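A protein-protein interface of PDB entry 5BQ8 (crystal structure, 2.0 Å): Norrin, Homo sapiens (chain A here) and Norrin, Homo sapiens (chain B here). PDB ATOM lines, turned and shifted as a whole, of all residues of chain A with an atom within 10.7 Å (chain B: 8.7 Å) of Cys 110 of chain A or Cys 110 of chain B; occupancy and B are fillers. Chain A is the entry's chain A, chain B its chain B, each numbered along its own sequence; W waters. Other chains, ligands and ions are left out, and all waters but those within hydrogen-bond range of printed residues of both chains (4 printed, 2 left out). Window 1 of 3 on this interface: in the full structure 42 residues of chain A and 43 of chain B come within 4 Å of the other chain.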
ATOM      1  N   CYS A  48       2.180  -5.545  18.541  1.00  0.00           N
ATOM      2  CA  CYS A  48       3.551  -5.461  18.995  1.00  0.00           C
ATOM      3  C   CYS A  48       3.714  -4.152  19.753  1.00  0.00           C
ATOM      4  O   CYS A  48       3.122  -3.137  19.388  1.00  0.00           O
ATOM      5  CB  CYS A  48       4.505  -5.554  17.809  1.00  0.00           C
ATOM      6  SG  CYS A  48       4.506  -7.190  17.047  1.00  0.00           S
ATOM      7  N   GLN A  50       6.378  -2.265  20.239  1.00  0.00           N
ATOM      8  CA  GLN A  50       7.229  -1.282  19.586  1.00  0.00           C
ATOM      9  C   GLN A  50       6.426  -0.426  18.618  1.00  0.00           C
ATOM     10  O   GLN A  50       5.609  -0.935  17.853  1.00  0.00           O
ATOM     11  CB  GLN A  50       8.360  -1.979  18.824  1.00  0.00           C
ATOM     12  CG  GLN A  50       9.182  -2.940  19.663  1.00  0.00           C
ATOM     13  CD  GLN A  50       8.661  -4.367  19.576  1.00  0.00           C
ATOM     14  OE1 GLN A  50       7.462  -4.591  19.418  1.00  0.00           O
ATOM     15  NE2 GLN A  50       9.562  -5.336  19.678  1.00  0.00           N
ATOM     16  N   ALA A  51       6.670   0.878  18.642  1.00  0.00           N
ATOM     17  CA  ALA A  51       6.098   1.760  17.641  1.00  0.00           C
ATOM     18  C   ALA A  51       6.754   1.452  16.302  1.00  0.00           C
ATOM     19  O   ALA A  51       7.907   1.021  16.260  1.00  0.00           O
ATOM     20  CB  ALA A  51       6.305   3.218  18.020  1.00  0.00           C
ATOM     21  N   SER A  52       6.020   1.668  15.215  1.00  0.00           N
ATOM     22  CA  SER A  52       6.592   1.577  13.880  1.00  0.00           C
ATOM     23  C   SER A  52       7.032   2.979  13.477  1.00  0.00           C
ATOM     24  O   SER A  52       6.436   3.962  13.910  1.00  0.00           O
ATOM     25  CB  SER A  52       5.585   0.989  12.889  1.00  0.00           C
ATOM     26  OG  SER A  52       4.447   1.826  12.756  1.00  0.00           O
ATOM     27  N   ARG A  53       8.065   3.081  12.651  1.00  0.00           N
ATOM     28  CA  ARG A  53       8.612   4.389  12.321  1.00  0.00           C
ATOM     29  C   ARG A  53       9.272   4.401  10.957  1.00  0.00           C
ATOM     30  O   ARG A  53       9.659   3.359  10.420  1.00  0.00           O
ATOM     31  CB  ARG A  53       9.627   4.803  13.384  1.00  0.00           C
ATOM     32  CG  ARG A  53      10.861   3.923  13.389  1.00  0.00           C
ATOM     33  CD  ARG A  53      11.834   4.314  14.469  1.00  0.00           C
ATOM     34  NE  ARG A  53      11.204   4.214  15.780  1.00  0.00           N
ATOM     35  CZ  ARG A  53      11.768   4.601  16.916  1.00  0.00           C
ATOM     36  NH1 ARG A  53      12.985   5.126  16.908  1.00  0.00           N
ATOM     37  NH2 ARG A  53      11.112   4.459  18.060  1.00  0.00           N
ATOM     38  N   SER A  54       9.382   5.594  10.390  1.00  0.00           N
ATOM     39  CA  SER A  54      10.072   5.767   9.129  1.00  0.00           C
ATOM     40  C   SER A  54      10.635   7.173   9.042  1.00  0.00           C
ATOM     41  O   SER A  54       9.929   8.145   9.320  1.00  0.00           O
ATOM     42  CB  SER A  54       9.139   5.499   7.954  1.00  0.00           C
ATOM     43  OG  SER A  54       9.806   5.722   6.724  1.00  0.00           O
ATOM     44  N   ARG A  69      14.321   5.089   5.877  1.00  0.00           N
ATOM     45  CA  ARG A  69      14.769   4.036   6.762  1.00  0.00           C
ATOM     46  C   ARG A  69      13.587   3.732   7.691  1.00  0.00           C
ATOM     47  O   ARG A  69      13.081   4.640   8.353  1.00  0.00           O
ATOM     48  CB  ARG A  69      15.996   4.486   7.557  1.00  0.00           C
ATOM     49  CG  ARG A  69      16.483   3.440   8.523  1.00  0.00           C
ATOM     50  CD  ARG A  69      17.647   3.862   9.409  1.00  0.00           C
ATOM     51  NE  ARG A  69      17.329   4.955  10.341  1.00  0.00           N
ATOM     52  CZ  ARG A  69      16.677   4.767  11.496  1.00  0.00           C
ATOM     53  NH1 ARG A  69      16.175   3.562  11.761  1.00  0.00           N
ATOM     54  NH2 ARG A  69      16.426   5.780  12.331  1.00  0.00           N
ATOM     55  N   SER A  70      13.147   2.477   7.748  1.00  0.00           N
ATOM     56  CA  SER A  70      11.926   2.137   8.477  1.00  0.00           C
ATOM     57  C   SER A  70      12.078   0.992   9.473  1.00  0.00           C
ATOM     58  O   SER A  70      12.959   0.142   9.342  1.00  0.00           O
ATOM     59  CB  SER A  70      10.821   1.769   7.489  1.00  0.00           C
ATOM     60  OG  SER A  70      10.523   2.847   6.617  1.00  0.00           O
ATOM     61  N   SER A  71      11.196   0.987  10.467  1.00  0.00           N
ATOM     62  CA  SER A  71      11.116  -0.080  11.452  1.00  0.00           C
ATOM     63  C   SER A  71       9.645  -0.353  11.732  1.00  0.00           C
ATOM     64  O   SER A  71       8.848   0.577  11.861  1.00  0.00           O
ATOM     65  CB  SER A  71      11.851   0.297  12.737  1.00  0.00           C
ATOM     66  OG  SER A  71      11.797  -0.748  13.693  1.00  0.00           O
ATOM     67  N   CYS A  72       9.286  -1.630  11.813  1.00  0.00           N
ATOM     68  CA  CYS A  72       7.903  -2.030  12.039  1.00  0.00           C
ATOM     69  C   CYS A  72       7.842  -3.477  12.496  1.00  0.00           C
ATOM     70  O   CYS A  72       8.381  -4.367  11.835  1.00  0.00           O
ATOM     71  CB  CYS A  72       7.068  -1.853  10.774  1.00  0.00           C
ATOM     72  SG  CYS A  72       5.357  -2.370  10.986  1.00  0.00           S
ATOM     73  N   HIS A  73       7.167  -3.713  13.612  1.00  0.00           N
ATOM     74  CA  HIS A  73       7.109  -5.047  14.188  1.00  0.00           C
ATOM     75  C   HIS A  73       5.755  -5.701  13.974  1.00  0.00           C
ATOM     76  O   HIS A  73       4.704  -5.089  14.177  1.00  0.00           O
ATOM     77  CB  HIS A  73       7.448  -4.988  15.675  1.00  0.00           C
ATOM     78  CG  HIS A  73       8.919  -4.918  15.944  1.00  0.00           C
ATOM     79  ND1 HIS A  73       9.647  -3.757  15.809  1.00  0.00           N
ATOM     80  CD2 HIS A  73       9.800  -5.874  16.323  1.00  0.00           C
ATOM     81  CE1 HIS A  73      10.915  -3.997  16.101  1.00  0.00           C
ATOM     82  NE2 HIS A  73      11.032  -5.273  16.416  1.00  0.00           N
ATOM     83  N   CYS A  74       5.807  -6.964  13.567  1.00  0.00           N
ATOM     84  CA  CYS A  74       4.624  -7.720  13.194  1.00  0.00           C
ATOM     85  C   CYS A  74       4.585  -9.016  13.984  1.00  0.00           C
ATOM     86  O   CYS A  74       5.616  -9.642  14.228  1.00  0.00           O
ATOM     87  CB  CYS A  74       4.631  -8.010  11.692  1.00  0.00           C
ATOM     88  SG  CYS A  74       4.897  -6.542  10.656  1.00  0.00           S
ATOM     89  N   CYS A  75       3.382  -9.414  14.377  1.00  0.00           N
ATOM     90  CA  CYS A  75       3.205 -10.637  15.144  1.00  0.00           C
ATOM     91  C   CYS A  75       3.251 -11.806  14.170  1.00  0.00           C
ATOM     92  O   CYS A  75       2.358 -11.955  13.335  1.00  0.00           O
ATOM     93  CB  CYS A  75       1.888 -10.603  15.919  1.00  0.00           C
ATOM     94  SG  CYS A  75       1.664 -11.940  17.119  1.00  0.00           S
ATOM     95  N   ARG A  76       4.307 -12.611  14.259  1.00  0.00           N
ATOM     96  CA  ARG A  76       4.538 -13.668  13.287  1.00  0.00           C
ATOM     97  C   ARG A  76       4.966 -14.977  13.942  1.00  0.00           C
ATOM     98  O   ARG A  76       5.361 -14.989  15.109  1.00  0.00           O
ATOM     99  CB  ARG A  76       5.599 -13.233  12.283  1.00  0.00           C
ATOM    100  CG  ARG A  76       5.158 -12.131  11.339  1.00  0.00           C
ATOM    101  CD  ARG A  76       6.272 -11.832  10.351  1.00  0.00           C
ATOM    102  NE  ARG A  76       5.901 -10.831   9.357  1.00  0.00           N
ATOM    103  CZ  ARG A  76       6.774 -10.144   8.627  1.00  0.00           C
ATOM    104  NH1 ARG A  76       8.077 -10.352   8.765  1.00  0.00           N
ATOM    105  NH2 ARG A  76       6.344  -9.255   7.744  1.00  0.00           N
ATOM    106  N   HIS A 106       6.017 -14.454  17.865  1.00  0.00           N
ATOM    107  CA  HIS A 106       6.841 -13.360  18.357  1.00  0.00           C
ATOM    108  C   HIS A 106       6.762 -12.156  17.433  1.00  0.00           C
ATOM    109  O   HIS A 106       6.339 -12.268  16.281  1.00  0.00           O
ATOM    110  CB  HIS A 106       8.297 -13.807  18.490  1.00  0.00           C
ATOM    111  CG  HIS A 106       8.978 -14.054  17.178  1.00  0.00           C
ATOM    112  ND1 HIS A 106      10.339 -13.919  17.011  1.00  0.00           N
ATOM    113  CD2 HIS A 106       8.487 -14.429  15.972  1.00  0.00           C
ATOM    114  CE1 HIS A 106      10.657 -14.198  15.759  1.00  0.00           C
ATOM    115  NE2 HIS A 106       9.551 -14.512  15.108  1.00  0.00           N
ATOM    116  N   CYS A 107       7.196 -11.008  17.942  1.00  0.00           N
ATOM    117  CA  CYS A 107       7.207  -9.786  17.153  1.00  0.00           C
ATOM    118  C   CYS A 107       8.552  -9.656  16.458  1.00  0.00           C
ATOM    119  O   CYS A 107       9.600  -9.785  17.091  1.00  0.00           O
ATOM    120  CB  CYS A 107       6.935  -8.562  18.029  1.00  0.00           C
ATOM    121  SG  CYS A 107       5.210  -8.387  18.528  1.00  0.00           S
ATOM    122  N   GLU A 108       8.515  -9.425  15.152  1.00  0.00           N
ATOM    123  CA  GLU A 108       9.729  -9.348  14.350  1.00  0.00           C
ATOM    124  C   GLU A 108       9.571  -8.248  13.313  1.00  0.00           C
ATOM    125  O   GLU A 108       8.454  -7.868  12.962  1.00  0.00           O
ATOM    126  CB  GLU A 108      10.040 -10.689  13.677  1.00  0.00           C
ATOM    127  CG  GLU A 108       9.129 -11.044  12.514  1.00  0.00           C
ATOM    128  CD  GLU A 108       9.538 -12.330  11.829  1.00  0.00           C
ATOM    129  OE1 GLU A 108       9.351 -12.422  10.602  1.00  0.00           O
ATOM    130  OE2 GLU A 108      10.046 -13.243  12.513  1.00  0.00           O
ATOM    131  N   GLU A 109      10.697  -7.744  12.823  1.00  0.00           N
ATOM    132  CA  GLU A 109      10.693  -6.678  11.837  1.00  0.00           C
ATOM    133  C   GLU A 109       9.935  -7.066  10.571  1.00  0.00           C
ATOM    134  O   GLU A 109      10.057  -8.190  10.085  1.00  0.00           O
ATOM    135  CB  GLU A 109      12.131  -6.302  11.471  1.00  0.00           C
ATOM    136  CG  GLU A 109      12.793  -5.355  12.446  1.00  0.00           C
ATOM    137  CD  GLU A 109      12.251  -3.945  12.337  1.00  0.00           C
ATOM    138  OE1 GLU A 109      11.449  -3.682  11.414  1.00  0.00           O
ATOM    139  OE2 GLU A 109      12.630  -3.102  13.173  1.00  0.00           O
ATOM    140  N   CYS A 110       9.156  -6.119  10.052  1.00  0.00           N
ATOM    141  CA  CYS A 110       8.450  -6.273   8.782  1.00  0.00           C
ATOM    142  C   CYS A 110       9.344  -6.865   7.697  1.00  0.00           C
ATOM    143  O   CYS A 110       9.000  -7.864   7.063  1.00  0.00           O
ATOM    144  CB  CYS A 110       7.925  -4.903   8.330  1.00  0.00           C
ATOM    145  SG  CYS A 110       7.409  -4.788   6.604  1.00  0.00           S
ATOM    146  N   ASN A 111      10.495  -6.226   7.506  1.00  0.00           N
ATOM    147  CA  ASN A 111      11.498  -6.627   6.522  1.00  0.00           C
ATOM    148  C   ASN A 111      12.645  -7.378   7.186  1.00  0.00           C
ATOM    149  O   ASN A 111      13.638  -6.770   7.586  1.00  0.00           O
ATOM    150  CB  ASN A 111      12.019  -5.408   5.762  1.00  0.00           C
ATOM    151  CG  ASN A 111      10.951  -4.764   4.893  1.00  0.00           C
ATOM    152  OD1 ASN A 111      10.111  -5.453   4.313  1.00  0.00           O
ATOM    153  ND2 ASN A 111      10.976  -3.439   4.806  1.00  0.00           N
ATOM    154  N   SER A 112      12.515  -8.696   7.285  1.00  0.00           N
ATOM    155  CA  SER A 112      13.447  -9.508   8.060  1.00  0.00           C
ATOM    156  C   SER A 112      14.043 -10.659   7.255  1.00  0.00           C
ATOM    157  O   SER A 112      14.963 -11.332   7.719  1.00  0.00           O
ATOM    158  CB  SER A 112      12.739 -10.061   9.299  1.00  0.00           C
ATOM    159  OG  SER A 112      11.726 -10.980   8.927  1.00  0.00           O
ATOM    160  N   GLY A 113      13.515 -10.897   6.058  1.00  0.00           N
ATOM    161  CA  GLY A 113      14.039 -11.950   5.204  1.00  0.00           C
ATOM    162  C   GLY A 113      13.545 -13.324   5.614  1.00  0.00           C
ATOM    163  O   GLY A 113      14.014 -14.344   5.105  1.00  0.00           O
ATOM    164  N   THR A 114      12.596 -13.344   6.542  1.00  0.00           N
ATOM    165  CA  THR A 114      12.048 -14.590   7.066  1.00  0.00           C
ATOM    166  C   THR A 114      11.050 -15.152   6.037  1.00  0.00           C
ATOM    167  O   THR A 114      10.686 -14.458   5.087  1.00  0.00           O
ATOM    168  CB  THR A 114      11.407 -14.332   8.471  1.00  0.00           C
ATOM    169  OG1 THR A 114      12.081 -15.115   9.463  1.00  0.00           O
ATOM    170  CG2 THR A 114       9.929 -14.642   8.513  1.00  0.00           C
ATOM    171  N   GLU A 115      10.619 -16.400   6.214  1.00  0.00           N
ATOM    172  CA  GLU A 115       9.721 -17.047   5.252  1.00  0.00           C
ATOM    173  C   GLU A 115       8.342 -16.378   5.204  1.00  0.00           C
ATOM    174  O   GLU A 115       7.615 -16.493   4.217  1.00  0.00           O
ATOM    175  CB  GLU A 115       9.576 -18.540   5.579  1.00  0.00           C
ATOM    176  CG  GLU A 115       8.939 -18.843   6.931  1.00  0.00           C
ATOM    177  CD  GLU A 115       8.943 -20.329   7.263  1.00  0.00           C
ATOM    178  OE1 GLU A 115       8.664 -20.682   8.429  1.00  0.00           O
ATOM    179  OE2 GLU A 115       9.219 -21.144   6.358  1.00  0.00           O
ATOM    180  N   THR A 116       8.000 -15.686   6.284  1.00  0.00           N
ATOM    181  CA  THR A 116       6.774 -14.901   6.392  1.00  0.00           C
ATOM    182  C   THR A 116       6.880 -13.555   5.657  1.00  0.00           C
ATOM    183  O   THR A 116       5.863 -12.947   5.317  1.00  0.00           O
ATOM    184  CB  THR A 116       6.426 -14.636   7.870  1.00  0.00           C
ATOM    185  OG1 THR A 116       6.727 -15.799   8.652  1.00  0.00           O
ATOM    186  CG2 THR A 116       4.955 -14.280   8.030  1.00  0.00           C
ATOM    187  N   SER A 117       8.106 -13.090   5.424  1.00  0.00           N
ATOM    188  CA  SER A 117       8.330 -11.807   4.752  1.00  0.00           C
ATOM    189  C   SER A 117       8.039 -11.898   3.256  1.00  0.00           C
ATOM    190  O   SER A 117       7.748 -12.973   2.732  1.00  0.00           O
ATOM    191  CB  SER A 117       9.773 -11.336   4.956  1.00  0.00           C
ATOM    192  OG  SER A 117      10.097 -11.230   6.330  1.00  0.00           O
ATOM    193  N   CYS B  48       0.045   1.805  14.946  1.00  0.00           N
ATOM    194  CA  CYS B  48      -1.103   1.615  14.081  1.00  0.00           C
ATOM    195  C   CYS B  48      -2.162   0.841  14.859  1.00  0.00           C
ATOM    196  O   CYS B  48      -1.837  -0.012  15.684  1.00  0.00           O
ATOM    197  CB  CYS B  48      -0.700   0.876  12.801  1.00  0.00           C
ATOM    198  SG  CYS B  48       0.362   1.848  11.677  1.00  0.00           S
ATOM    199  N   SER B  52      -1.596  -6.945  14.105  1.00  0.00           N
ATOM    200  CA  SER B  52      -0.924  -7.713  13.074  1.00  0.00           C
ATOM    201  C   SER B  52      -1.237  -9.177  13.325  1.00  0.00           C
ATOM    202  O   SER B  52      -1.495  -9.583  14.462  1.00  0.00           O
ATOM    203  CB  SER B  52       0.584  -7.455  13.071  1.00  0.00           C
ATOM    204  OG  SER B  52       1.195  -7.879  14.281  1.00  0.00           O
ATOM    205  N   SER B  70      -0.085 -13.264   6.066  1.00  0.00           N
ATOM    206  CA  SER B  70       0.082 -12.328   7.168  1.00  0.00           C
ATOM    207  C   SER B  70      -0.422 -10.925   6.847  1.00  0.00           C
ATOM    208  O   SER B  70      -0.534 -10.532   5.686  1.00  0.00           O
ATOM    209  CB  SER B  70       1.555 -12.276   7.582  1.00  0.00           C
ATOM    210  OG  SER B  70       2.332 -11.561   6.641  1.00  0.00           O
ATOM    211  N   SER B  71      -0.735 -10.187   7.907  1.00  0.00           N
ATOM    212  CA  SER B  71      -1.157  -8.796   7.815  1.00  0.00           C
ATOM    213  C   SER B  71      -0.473  -8.017   8.928  1.00  0.00           C
ATOM    214  O   SER B  71      -0.364  -8.502  10.051  1.00  0.00           O
ATOM    215  CB  SER B  71      -2.678  -8.674   7.928  1.00  0.00           C
ATOM    216  OG  SER B  71      -3.091  -7.325   7.825  1.00  0.00           O
ATOM    217  N   CYS B  72       0.009  -6.822   8.604  1.00  0.00           N
ATOM    218  CA  CYS B  72       0.739  -5.999   9.557  1.00  0.00           C
ATOM    219  C   CYS B  72       0.808  -4.562   9.071  1.00  0.00           C
ATOM    220  O   CYS B  72       1.230  -4.308   7.948  1.00  0.00           O
ATOM    221  CB  CYS B  72       2.151  -6.541   9.771  1.00  0.00           C
ATOM    222  SG  CYS B  72       3.137  -5.563  10.921  1.00  0.00           S
ATOM    223  N   HIS B  73       0.417  -3.625   9.925  1.00  0.00           N
ATOM    224  CA  HIS B  73       0.362  -2.221   9.539  1.00  0.00           C
ATOM    225  C   HIS B  73       1.515  -1.426  10.140  1.00  0.00           C
ATOM    226  O   HIS B  73       1.835  -1.566  11.320  1.00  0.00           O
ATOM    227  CB  HIS B  73      -0.987  -1.622   9.950  1.00  0.00           C
ATOM    228  CG  HIS B  73      -2.093  -1.962   9.001  1.00  0.00           C
ATOM    229  ND1 HIS B  73      -2.729  -3.185   9.007  1.00  0.00           N
ATOM    230  CD2 HIS B  73      -2.645  -1.257   7.986  1.00  0.00           C
ATOM    231  CE1 HIS B  73      -3.639  -3.210   8.051  1.00  0.00           C
ATOM    232  NE2 HIS B  73      -3.607  -2.053   7.416  1.00  0.00           N
ATOM    233  N   CYS B  74       2.133  -0.596   9.300  1.00  0.00           N
ATOM    234  CA  CYS B  74       3.319   0.167   9.672  1.00  0.00           C
ATOM    235  C   CYS B  74       3.127   1.646   9.400  1.00  0.00           C
ATOM    236  O   CYS B  74       2.536   2.033   8.389  1.00  0.00           O
ATOM    237  CB  CYS B  74       4.548  -0.330   8.907  1.00  0.00           C
ATOM    238  SG  CYS B  74       4.837  -2.104   9.043  1.00  0.00           S
ATOM    239  N   CYS B  75       3.652   2.466  10.301  1.00  0.00           N
ATOM    240  CA  CYS B  75       3.551   3.909  10.157  1.00  0.00           C
ATOM    241  C   CYS B  75       4.627   4.377   9.186  1.00  0.00           C
ATOM    242  O   CYS B  75       5.814   4.373   9.512  1.00  0.00           O
ATOM    243  CB  CYS B  75       3.698   4.592  11.514  1.00  0.00           C
ATOM    244  SG  CYS B  75       3.322   6.351  11.503  1.00  0.00           S
ATOM    245  N   ARG B  76       4.197   4.793   7.999  1.00  0.00           N
ATOM    246  CA  ARG B  76       5.108   5.124   6.908  1.00  0.00           C
ATOM    247  C   ARG B  76       4.675   6.407   6.209  1.00  0.00           C
ATOM    248  O   ARG B  76       3.535   6.850   6.377  1.00  0.00           O
ATOM    249  CB  ARG B  76       5.152   3.984   5.898  1.00  0.00           C
ATOM    250  CG  ARG B  76       5.830   2.722   6.391  1.00  0.00           C
ATOM    251  CD  ARG B  76       5.799   1.673   5.306  1.00  0.00           C
ATOM    252  NE  ARG B  76       6.480   0.452   5.703  1.00  0.00           N
ATOM    253  CZ  ARG B  76       6.271  -0.741   5.157  1.00  0.00           C
ATOM    254  NH1 ARG B  76       5.379  -0.883   4.187  1.00  0.00           N
ATOM    255  NH2 ARG B  76       6.950  -1.796   5.597  1.00  0.00           N
ATOM    256  N   CYS B 107      -0.891   4.547   8.153  1.00  0.00           N
ATOM    257  CA  CYS B 107      -0.608   3.153   8.446  1.00  0.00           C
ATOM    258  C   CYS B 107      -0.820   2.330   7.191  1.00  0.00           C
ATOM    259  O   CYS B 107      -1.847   2.440   6.522  1.00  0.00           O
ATOM    260  CB  CYS B 107      -1.490   2.657   9.587  1.00  0.00           C
ATOM    261  SG  CYS B 107      -0.978   3.290  11.185  1.00  0.00           S
ATOM    262  N   GLU B 108       0.173   1.512   6.870  1.00  0.00           N
ATOM    263  CA  GLU B 108       0.162   0.762   5.628  1.00  0.00           C
ATOM    264  C   GLU B 108       0.679  -0.650   5.841  1.00  0.00           C
ATOM    265  O   GLU B 108       1.473  -0.900   6.745  1.00  0.00           O
ATOM    266  CB  GLU B 108       1.010   1.498   4.592  1.00  0.00           C
ATOM    267  CG  GLU B 108       1.069   0.854   3.234  1.00  0.00           C
ATOM    268  CD  GLU B 108       2.125   1.475   2.346  1.00  0.00           C
ATOM    269  OE1 GLU B 108       2.432   2.674   2.516  1.00  0.00           O
ATOM    270  OE2 GLU B 108       2.556   0.793   1.396  1.00  0.00           O
ATOM    271  N   GLU B 109       0.231  -1.570   4.996  1.00  0.00           N
ATOM    272  CA  GLU B 109       0.649  -2.959   5.096  1.00  0.00           C
ATOM    273  C   GLU B 109       2.152  -3.086   4.917  1.00  0.00           C
ATOM    274  O   GLU B 109       2.751  -2.436   4.059  1.00  0.00           O
ATOM    275  CB  GLU B 109      -0.087  -3.813   4.064  1.00  0.00           C
ATOM    276  CG  GLU B 109      -1.482  -4.230   4.514  1.00  0.00           C
ATOM    277  CD  GLU B 109      -1.463  -5.315   5.583  1.00  0.00           C
ATOM    278  OE1 GLU B 109      -0.376  -5.854   5.880  1.00  0.00           O
ATOM    279  OE2 GLU B 109      -2.540  -5.620   6.138  1.00  0.00           O
ATOM    280  N   CYS B 110       2.741  -3.928   5.754  1.00  0.00           N
ATOM    281  CA  CYS B 110       4.157  -4.254   5.709  1.00  0.00           C
ATOM    282  C   CYS B 110       4.626  -4.550   4.282  1.00  0.00           C
ATOM    283  O   CYS B 110       5.625  -3.995   3.827  1.00  0.00           O
ATOM    284  CB  CYS B 110       4.418  -5.442   6.637  1.00  0.00           C
ATOM    285  SG  CYS B 110       6.007  -6.246   6.463  1.00  0.00           S
ATOM    286  N   ASN B 111       3.897  -5.419   3.586  1.00  0.00           N
ATOM    287  CA  ASN B 111       4.234  -5.796   2.214  1.00  0.00           C
ATOM    288  C   ASN B 111       3.401  -5.020   1.199  1.00  0.00           C
ATOM    289  O   ASN B 111       2.188  -5.212   1.096  1.00  0.00           O
ATOM    290  CB  ASN B 111       4.027  -7.299   2.010  1.00  0.00           C
ATOM    291  CG  ASN B 111       4.977  -8.140   2.846  1.00  0.00           C
ATOM    292  OD1 ASN B 111       6.136  -7.773   3.052  1.00  0.00           O
ATOM    293  ND2 ASN B 111       4.488  -9.272   3.337  1.00  0.00           N
HETATM  294  O   HOH W   1       3.361 -13.991   5.287  1.00  0.00           O
HETATM  295  O   HOH W   2       2.436   0.247  14.002  1.00  0.00           O
HETATM  296  O   HOH W   3       2.085 -10.320  11.101  1.00  0.00           O
HETATM  297  O   HOH W   4       1.806  -5.391  15.866  1.00  0.00           O
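SG of Cys 74 of chain A is disulfide-bonded to SG of Cys 72 of chain B.
The backbone carbonyl oxygen (O) of His 73 of chain B lies close to the side-chain sulfur (SG) of Cys 72 of chain A (3.6 Å).
The side-chain hydroxyl of Ser 52 of chain A lies within hydrogen-bond range of the backbone NH of Cys 75 of chain B.
O of His 73 of chain A lies close to SG of Cys 72 of chain B.
The backbone NH of Cys 75 of chain A is in hydrogen-bond range of the side-chain hydroxyl of Ser 52 of chain B (2.7 Å).
The side-chain sulfur (SG) of Cys 110 of chain A is disulfide-bonded to the side-chain sulfur (SG) of Cys 110 of chain B.
The guanidinium group (NH2) of Arg 76 of chain B sits at hydrogen-bond distance from the side-chain sulfur (SG) of Cys 110 of chain A (3.2 Å).
NH2 of Arg 76 of chain A is in hydrogen-bond range of SG of Cys 110 of chain B (3.3 Å).
The side-chain sulfur of Cys 72 of chain A forms a disulfide with the side-chain sulfur of Cys 74 of chain B (2.0 Å).
Among the printed residues, merely in contact across the chains: Ser 52 of chain A with Cys 74 of chain B (3.6 Å), Arg 53 of chain A with Cys 75 of chain B (3.7 Å), Ser 54 of chain A with Cys 75 of chain B (3.8 Å), Cys 72 of chain A with Cys 72 of chain B (3.9 Å), Cys 74 of chain A with Ser 52 of chain B (3.6 Å) and Thr 116 of chain A with Ser 70 of chain B (3.97 Å).
The guanidinium group of Arg 76 of chain A is in hydrogen-bond range of the backbone carbonyl oxygen of Glu 109 of chain A, at 3.2 Å.
The backbone carbonyl oxygen of Cys 72 of chain B lies within hydrogen-bond range of the backbone NH of Cys 110 of chain B, 2.7 Å away.
OE1 of Glu 109 of chain B is in hydrogen-bond range of N of Cys 72 of chain B.
The side-chain hydroxyl (OG) of Ser 70 of chain A is in hydrogen-bond range of the side-chain hydroxyl (OG) of Ser 54 of chain A, at 3.0 Å.
O of Cys 72 of chain A lies within hydrogen-bond range of N of Cys 110 of chain A, at 2.6 Å.
The side-chain sulfur of Cys 48 of chain A sits close to the backbone NH of Cys 74 of chain A (3.7 Å).
Printed residues of chain A that touch a printed residue of chain B: Ser 52, Arg 53, Ser 54, Cys 72, His 73, Cys 74, Cys 75, Arg 76, Cys 110 and Thr 116.
Among the printed residues, 15 pairs touch across the chains.
Of the printed residues of chain B, Ser 54 of chain A touches Cys 75.
No residue of chain B comes within 4 Å of Asn 111 of chain A.
Of the printed residues of chain A, Ser 52 of chain B touches Cys 74 and Cys 75.
Of the printed residues of chain A, Cys 72 of chain B touches Cys 72, His 73 and Cys 74.
Of the printed residues of chain A, His 73 of chain B touches Cys 72.
No residue of chain A comes within 4 Å of Glu 109 of chain B.
Cys 110 of chain B touches just these residues of chain A: Arg 76 and Cys 110.
No residue of chain A comes within 4 Å of Asn 111 of chain B.
Water W4 lies within hydrogen-bond range of the backbone NH (N) of Cys 48 of chain A (2.7 Å), the side-chain hydroxyl (OG) of Ser 52 of chain B (3.0 Å) and the backbone carbonyl oxygen (O) of His 73 of chain A (3.4 Å).
Water W1 lies within hydrogen-bond range of O of Thr 116 of chain A (2.7 Å) and OG of Ser 70 of chain B (3.0 Å).
Water W3 lies within hydrogen-bond range of the backbone carbonyl oxygen of Cys 75 of chain A (2.8 Å) and the backbone carbonyl oxygen of Ser 71 of chain B (3.2 Å).
Water W2 lies within hydrogen-bond range of OG of Ser 52 of chain A (2.8 Å), N of Cys 48 of chain B (3.0 Å) and O of His 73 of chain B (3.3 Å).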
